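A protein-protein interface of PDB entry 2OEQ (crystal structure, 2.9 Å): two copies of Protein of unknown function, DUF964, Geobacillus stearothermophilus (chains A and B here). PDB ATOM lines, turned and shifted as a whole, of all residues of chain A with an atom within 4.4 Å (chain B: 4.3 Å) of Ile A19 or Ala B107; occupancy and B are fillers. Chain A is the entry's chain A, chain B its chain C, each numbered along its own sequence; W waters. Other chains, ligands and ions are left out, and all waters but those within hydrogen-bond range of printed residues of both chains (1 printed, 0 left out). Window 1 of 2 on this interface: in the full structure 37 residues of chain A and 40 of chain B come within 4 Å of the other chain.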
ATOM      1  N   LEU A  15       0.104 -22.276 -19.724  1.00  0.00           N
ATOM      2  CA  LEU A  15       0.575 -21.044 -20.336  1.00  0.00           C
ATOM      3  C   LEU A  15       1.061 -21.277 -21.743  1.00  0.00           C
ATOM      4  O   LEU A  15       0.848 -20.433 -22.609  1.00  0.00           O
ATOM      5  CB  LEU A  15       1.712 -20.430 -19.512  1.00  0.00           C
ATOM      6  CG  LEU A  15       2.333 -19.069 -19.880  1.00  0.00           C
ATOM      7  CD1 LEU A  15       1.421 -17.936 -19.551  1.00  0.00           C
ATOM      8  CD2 LEU A  15       3.600 -18.916 -19.107  1.00  0.00           C
ATOM      9  N   GLU A  16       1.726 -22.410 -21.970  1.00  0.00           N
ATOM     10  CA  GLU A  16       2.244 -22.749 -23.303  1.00  0.00           C
ATOM     11  C   GLU A  16       1.087 -22.883 -24.309  1.00  0.00           C
ATOM     12  O   GLU A  16       1.119 -22.366 -25.430  1.00  0.00           O
ATOM     13  CB  GLU A  16       3.024 -24.045 -23.234  1.00  0.00           C
ATOM     14  CG  GLU A  16       3.539 -24.481 -24.561  1.00  0.00           C
ATOM     15  CD  GLU A  16       4.278 -25.807 -24.487  1.00  0.00           C
ATOM     16  OE1 GLU A  16       5.014 -26.163 -25.447  1.00  0.00           O
ATOM     17  OE2 GLU A  16       4.118 -26.500 -23.461  1.00  0.00           O
ATOM     18  N   GLN A  17       0.059 -23.581 -23.864  1.00  0.00           N
ATOM     19  CA  GLN A  17      -1.127 -23.815 -24.639  1.00  0.00           C
ATOM     20  C   GLN A  17      -1.745 -22.438 -24.913  1.00  0.00           C
ATOM     21  O   GLN A  17      -1.951 -22.045 -26.068  1.00  0.00           O
ATOM     22  CB  GLN A  17      -2.054 -24.688 -23.805  1.00  0.00           C
ATOM     23  CG  GLN A  17      -3.149 -25.413 -24.541  1.00  0.00           C
ATOM     24  CD  GLN A  17      -3.918 -26.336 -23.612  1.00  0.00           C
ATOM     25  OE1 GLN A  17      -3.316 -27.111 -22.866  1.00  0.00           O
ATOM     26  NE2 GLN A  17      -5.249 -26.258 -23.647  1.00  0.00           N
ATOM     27  N   ALA A  18      -2.025 -21.698 -23.842  1.00  0.00           N
ATOM     28  CA  ALA A  18      -2.625 -20.358 -23.948  1.00  0.00           C
ATOM     29  C   ALA A  18      -1.875 -19.462 -24.920  1.00  0.00           C
ATOM     30  O   ALA A  18      -2.473 -18.766 -25.739  1.00  0.00           O
ATOM     31  CB  ALA A  18      -2.664 -19.688 -22.568  1.00  0.00           C
ATOM     32  N   ILE A  19      -0.557 -19.476 -24.802  1.00  0.00           N
ATOM     33  CA  ILE A  19       0.253 -18.663 -25.654  1.00  0.00           C
ATOM     34  C   ILE A  19      -0.009 -19.070 -27.092  1.00  0.00           C
ATOM     35  O   ILE A  19      -0.568 -18.300 -27.877  1.00  0.00           O
ATOM     36  CB  ILE A  19       1.739 -18.829 -25.315  1.00  0.00           C
ATOM     37  CG1 ILE A  19       2.047 -18.127 -23.990  1.00  0.00           C
ATOM     38  CG2 ILE A  19       2.605 -18.237 -26.426  1.00  0.00           C
ATOM     39  CD1 ILE A  19       3.462 -18.365 -23.446  1.00  0.00           C
ATOM     40  N   ARG A  20       0.384 -20.295 -27.418  1.00  0.00           N
ATOM     41  CA  ARG A  20       0.230 -20.844 -28.755  1.00  0.00           C
ATOM     42  C   ARG A  20      -1.161 -20.596 -29.348  1.00  0.00           C
ATOM     43  O   ARG A  20      -1.321 -20.459 -30.547  1.00  0.00           O
ATOM     44  CB  ARG A  20       0.532 -22.342 -28.707  1.00  0.00           C
ATOM     45  CG  ARG A  20       0.644 -22.972 -30.060  1.00  0.00           C
ATOM     46  CD  ARG A  20       0.973 -24.447 -29.976  1.00  0.00           C
ATOM     47  NE  ARG A  20       2.381 -24.731 -29.702  1.00  0.00           N
ATOM     48  CZ  ARG A  20       2.837 -25.189 -28.537  1.00  0.00           C
ATOM     49  NH1 ARG A  20       1.997 -25.411 -27.529  1.00  0.00           N
ATOM     50  NH2 ARG A  20       4.133 -25.452 -28.383  1.00  0.00           N
ATOM     51  N   ALA A  21      -2.175 -20.509 -28.511  1.00  0.00           N
ATOM     52  CA  ALA A  21      -3.509 -20.305 -29.033  1.00  0.00           C
ATOM     53  C   ALA A  21      -3.937 -18.847 -29.165  1.00  0.00           C
ATOM     54  O   ALA A  21      -4.924 -18.555 -29.839  1.00  0.00           O
ATOM     55  CB  ALA A  21      -4.517 -21.074 -28.152  1.00  0.00           C
ATOM     56  N   SER A  22      -3.204 -17.939 -28.523  1.00  0.00           N
ATOM     57  CA  SER A  22      -3.542 -16.512 -28.529  1.00  0.00           C
ATOM     58  C   SER A  22      -3.538 -15.923 -29.921  1.00  0.00           C
ATOM     59  O   SER A  22      -2.748 -16.343 -30.761  1.00  0.00           O
ATOM     60  CB  SER A  22      -2.543 -15.725 -27.683  1.00  0.00           C
ATOM     61  OG  SER A  22      -1.388 -15.425 -28.448  1.00  0.00           O
ATOM     62  N   PHE A  25      -0.046 -15.007 -31.556  1.00  0.00           N
ATOM     63  CA  PHE A  25       0.771 -16.077 -32.064  1.00  0.00           C
ATOM     64  C   PHE A  25       0.209 -16.633 -33.368  1.00  0.00           C
ATOM     65  O   PHE A  25       0.950 -17.042 -34.257  1.00  0.00           O
ATOM     66  CB  PHE A  25       0.857 -17.172 -31.020  1.00  0.00           C
ATOM     67  CG  PHE A  25       1.967 -18.099 -31.244  1.00  0.00           C
ATOM     68  CD1 PHE A  25       3.274 -17.680 -31.035  1.00  0.00           C
ATOM     69  CD2 PHE A  25       1.722 -19.395 -31.686  1.00  0.00           C
ATOM     70  CE1 PHE A  25       4.351 -18.545 -31.257  1.00  0.00           C
ATOM     71  CE2 PHE A  25       2.771 -20.292 -31.919  1.00  0.00           C
ATOM     72  CZ  PHE A  25       4.097 -19.882 -31.708  1.00  0.00           C
ATOM     73  N   LEU B   8      -1.064 -11.737 -24.000  1.00  0.00           N
ATOM     74  CA  LEU B   8       0.055 -12.426 -23.375  1.00  0.00           C
ATOM     75  C   LEU B   8       0.462 -11.812 -22.053  1.00  0.00           C
ATOM     76  O   LEU B   8       0.640 -12.526 -21.078  1.00  0.00           O
ATOM     77  CB  LEU B   8       1.230 -12.493 -24.330  1.00  0.00           C
ATOM     78  CG  LEU B   8       0.899 -13.254 -25.603  1.00  0.00           C
ATOM     79  CD1 LEU B   8       2.114 -13.330 -26.530  1.00  0.00           C
ATOM     80  CD2 LEU B   8       0.494 -14.624 -25.201  1.00  0.00           C
ATOM     81  N   VAL B 103       9.827 -22.869 -16.090  1.00  0.00           N
ATOM     82  CA  VAL B 103       8.538 -22.365 -16.524  1.00  0.00           C
ATOM     83  C   VAL B 103       8.753 -21.412 -17.671  1.00  0.00           C
ATOM     84  O   VAL B 103       8.096 -21.511 -18.701  1.00  0.00           O
ATOM     85  CB  VAL B 103       7.853 -21.589 -15.410  1.00  0.00           C
ATOM     86  CG1 VAL B 103       6.474 -21.092 -15.870  1.00  0.00           C
ATOM     87  CG2 VAL B 103       7.787 -22.457 -14.164  1.00  0.00           C
ATOM     88  N   GLN B 104       9.682 -20.478 -17.493  1.00  0.00           N
ATOM     89  CA  GLN B 104       9.919 -19.521 -18.554  1.00  0.00           C
ATOM     90  C   GLN B 104      10.415 -20.207 -19.824  1.00  0.00           C
ATOM     91  O   GLN B 104      10.159 -19.726 -20.926  1.00  0.00           O
ATOM     92  CB  GLN B 104      10.836 -18.369 -18.084  1.00  0.00           C
ATOM     93  CG  GLN B 104      12.168 -18.705 -17.503  1.00  0.00           C
ATOM     94  CD  GLN B 104      12.692 -17.580 -16.595  1.00  0.00           C
ATOM     95  OE1 GLN B 104      13.867 -17.573 -16.211  1.00  0.00           O
ATOM     96  NE2 GLN B 104      11.818 -16.636 -16.237  1.00  0.00           N
ATOM     97  N   GLN B 105      11.063 -21.359 -19.674  1.00  0.00           N
ATOM     98  CA  GLN B 105      11.545 -22.121 -20.823  1.00  0.00           C
ATOM     99  C   GLN B 105      10.334 -22.660 -21.608  1.00  0.00           C
ATOM    100  O   GLN B 105      10.326 -22.691 -22.841  1.00  0.00           O
ATOM    101  CB  GLN B 105      12.440 -23.272 -20.349  1.00  0.00           C
ATOM    102  CG  GLN B 105      12.876 -24.241 -21.440  1.00  0.00           C
ATOM    103  CD  GLN B 105      11.888 -25.387 -21.656  1.00  0.00           C
ATOM    104  OE1 GLN B 105      12.079 -26.227 -22.539  1.00  0.00           O
ATOM    105  NE2 GLN B 105      10.833 -25.428 -20.844  1.00  0.00           N
ATOM    106  N   ILE B 106       9.299 -23.074 -20.891  1.00  0.00           N
ATOM    107  CA  ILE B 106       8.135 -23.589 -21.557  1.00  0.00           C
ATOM    108  C   ILE B 106       7.468 -22.452 -22.279  1.00  0.00           C
ATOM    109  O   ILE B 106       6.976 -22.618 -23.385  1.00  0.00           O
ATOM    110  CB  ILE B 106       7.211 -24.282 -20.546  1.00  0.00           C
ATOM    111  CG1 ILE B 106       7.753 -25.688 -20.322  1.00  0.00           C
ATOM    112  CG2 ILE B 106       5.751 -24.330 -21.038  1.00  0.00           C
ATOM    113  CD1 ILE B 106       7.538 -26.227 -18.939  1.00  0.00           C
ATOM    114  N   ALA B 107       7.479 -21.281 -21.676  1.00  0.00           N
ATOM    115  CA  ALA B 107       6.868 -20.145 -22.330  1.00  0.00           C
ATOM    116  C   ALA B 107       7.544 -19.889 -23.658  1.00  0.00           C
ATOM    117  O   ALA B 107       6.953 -19.300 -24.560  1.00  0.00           O
ATOM    118  CB  ALA B 107       6.980 -18.914 -21.468  1.00  0.00           C
ATOM    119  N   MET B 108       8.785 -20.324 -23.787  1.00  0.00           N
ATOM    120  CA  MET B 108       9.508 -20.102 -25.031  1.00  0.00           C
ATOM    121  C   MET B 108       9.285 -21.151 -26.123  1.00  0.00           C
ATOM    122  O   MET B 108       9.733 -20.956 -27.252  1.00  0.00           O
ATOM    123  CB  MET B 108      11.012 -20.014 -24.759  1.00  0.00           C
ATOM    124  CG  MET B 108      11.607 -18.680 -25.045  1.00  0.00           C
ATOM    125  SD  MET B 108      11.359 -18.190 -26.866  1.00  0.00           S
ATOM    126  CE  MET B 108      13.107 -18.711 -27.506  1.00  0.00           C
ATOM    127  N   LYS B 109       8.606 -22.255 -25.817  1.00  0.00           N
ATOM    128  CA  LYS B 109       8.419 -23.299 -26.825  1.00  0.00           C
ATOM    129  C   LYS B 109       7.635 -22.890 -28.082  1.00  0.00           C
ATOM    130  O   LYS B 109       8.105 -23.034 -29.205  1.00  0.00           O
ATOM    131  CB  LYS B 109       7.773 -24.532 -26.187  1.00  0.00           C
ATOM    132  CG  LYS B 109       8.570 -25.087 -25.032  1.00  0.00           C
ATOM    133  CD  LYS B 109       8.092 -26.474 -24.660  1.00  0.00           C
ATOM    134  CE  LYS B 109       8.409 -27.485 -25.766  1.00  0.00           C
ATOM    135  NZ  LYS B 109       7.882 -28.875 -25.502  1.00  0.00           N
ATOM    136  N   PRO B 110       6.432 -22.363 -27.908  1.00  0.00           N
ATOM    137  CA  PRO B 110       5.711 -21.996 -29.121  1.00  0.00           C
ATOM    138  C   PRO B 110       6.578 -21.267 -30.124  1.00  0.00           C
ATOM    139  O   PRO B 110       6.542 -21.596 -31.315  1.00  0.00           O
ATOM    140  CB  PRO B 110       4.560 -21.158 -28.590  1.00  0.00           C
ATOM    141  CG  PRO B 110       4.245 -21.834 -27.315  1.00  0.00           C
ATOM    142  CD  PRO B 110       5.633 -22.079 -26.712  1.00  0.00           C
HETATM  143  O   HOH W   1       5.315 -29.011 -27.042  1.00  0.00           O
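The side-chain amino group of Lys B109 lies within salt-bridge range of the side-chain carboxylate of Glu A16, 3.9 Å away.
The backbone NH (N) of Phe A25 lies within hydrogen-bond range of the side-chain hydroxyl (OG) of Ser A22, at 3.4 Å. The side-chain hydroxyl of Ser A22 sits at hydrogen-bond distance from the backbone carbonyl oxygen of Ile A19, 3.0 Å away. OE1 of Glu A16 is in salt-bridge range of NH2 of Arg A20, 3.1 Å away.
Glu A16 touches Ile B106. O of Glu A16 touches CG of Pro B110, at 3.7 Å. Ile A19 touches Ala B107 (CD1 to O, 3.8 Å). Arg A20 touches Pro B110. CD2 of Leu B8 touches OG of Ser A22, at 3.8 Å. Pro B110 touches Phe A25.
Of the printed residues of chain B, Ile A19 touches Ala B107 (3.8 Å). Ala B107 touches just one residue of chain A: Ile A19 (3.8 Å). Of the printed residues of chain A, Pro B110 touches Glu A16, Arg A20 and Phe A25. Of the printed residues of chain A, Leu B8 touches Ser A22. Printed residues of chain A within 4 Å of Lys B109: Glu A16 (3.2 Å). The nearest printed residue of chain B that does not touch Glu A16 is Ala B107 (5.4 Å).
Printed residues of chain B that touch a printed residue of chain A: Leu B8, Ile B106, Ala B107, Lys B109 and Pro B110. Along chain B the printed residues that touch a printed residue of chain A span positions 8 to 110. Hydrophobic or aromatic side chains of chain A within 4 Å of the printed part of chain B: Ile A19 and Phe A25. Along chain A the printed residues that touch a printed residue of chain B span positions 16 to 25. Among the printed residues, 7 pairs touch across the chains.
No position is printed for both chains. Of the 7 pairs that touch across the chains among the printed residues, none has its exchanged pair printed and touching as well.
Water W1 lies within hydrogen-bond range of the side-chain amino group of Lys B109 and the side-chain carboxylate of Glu A16.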
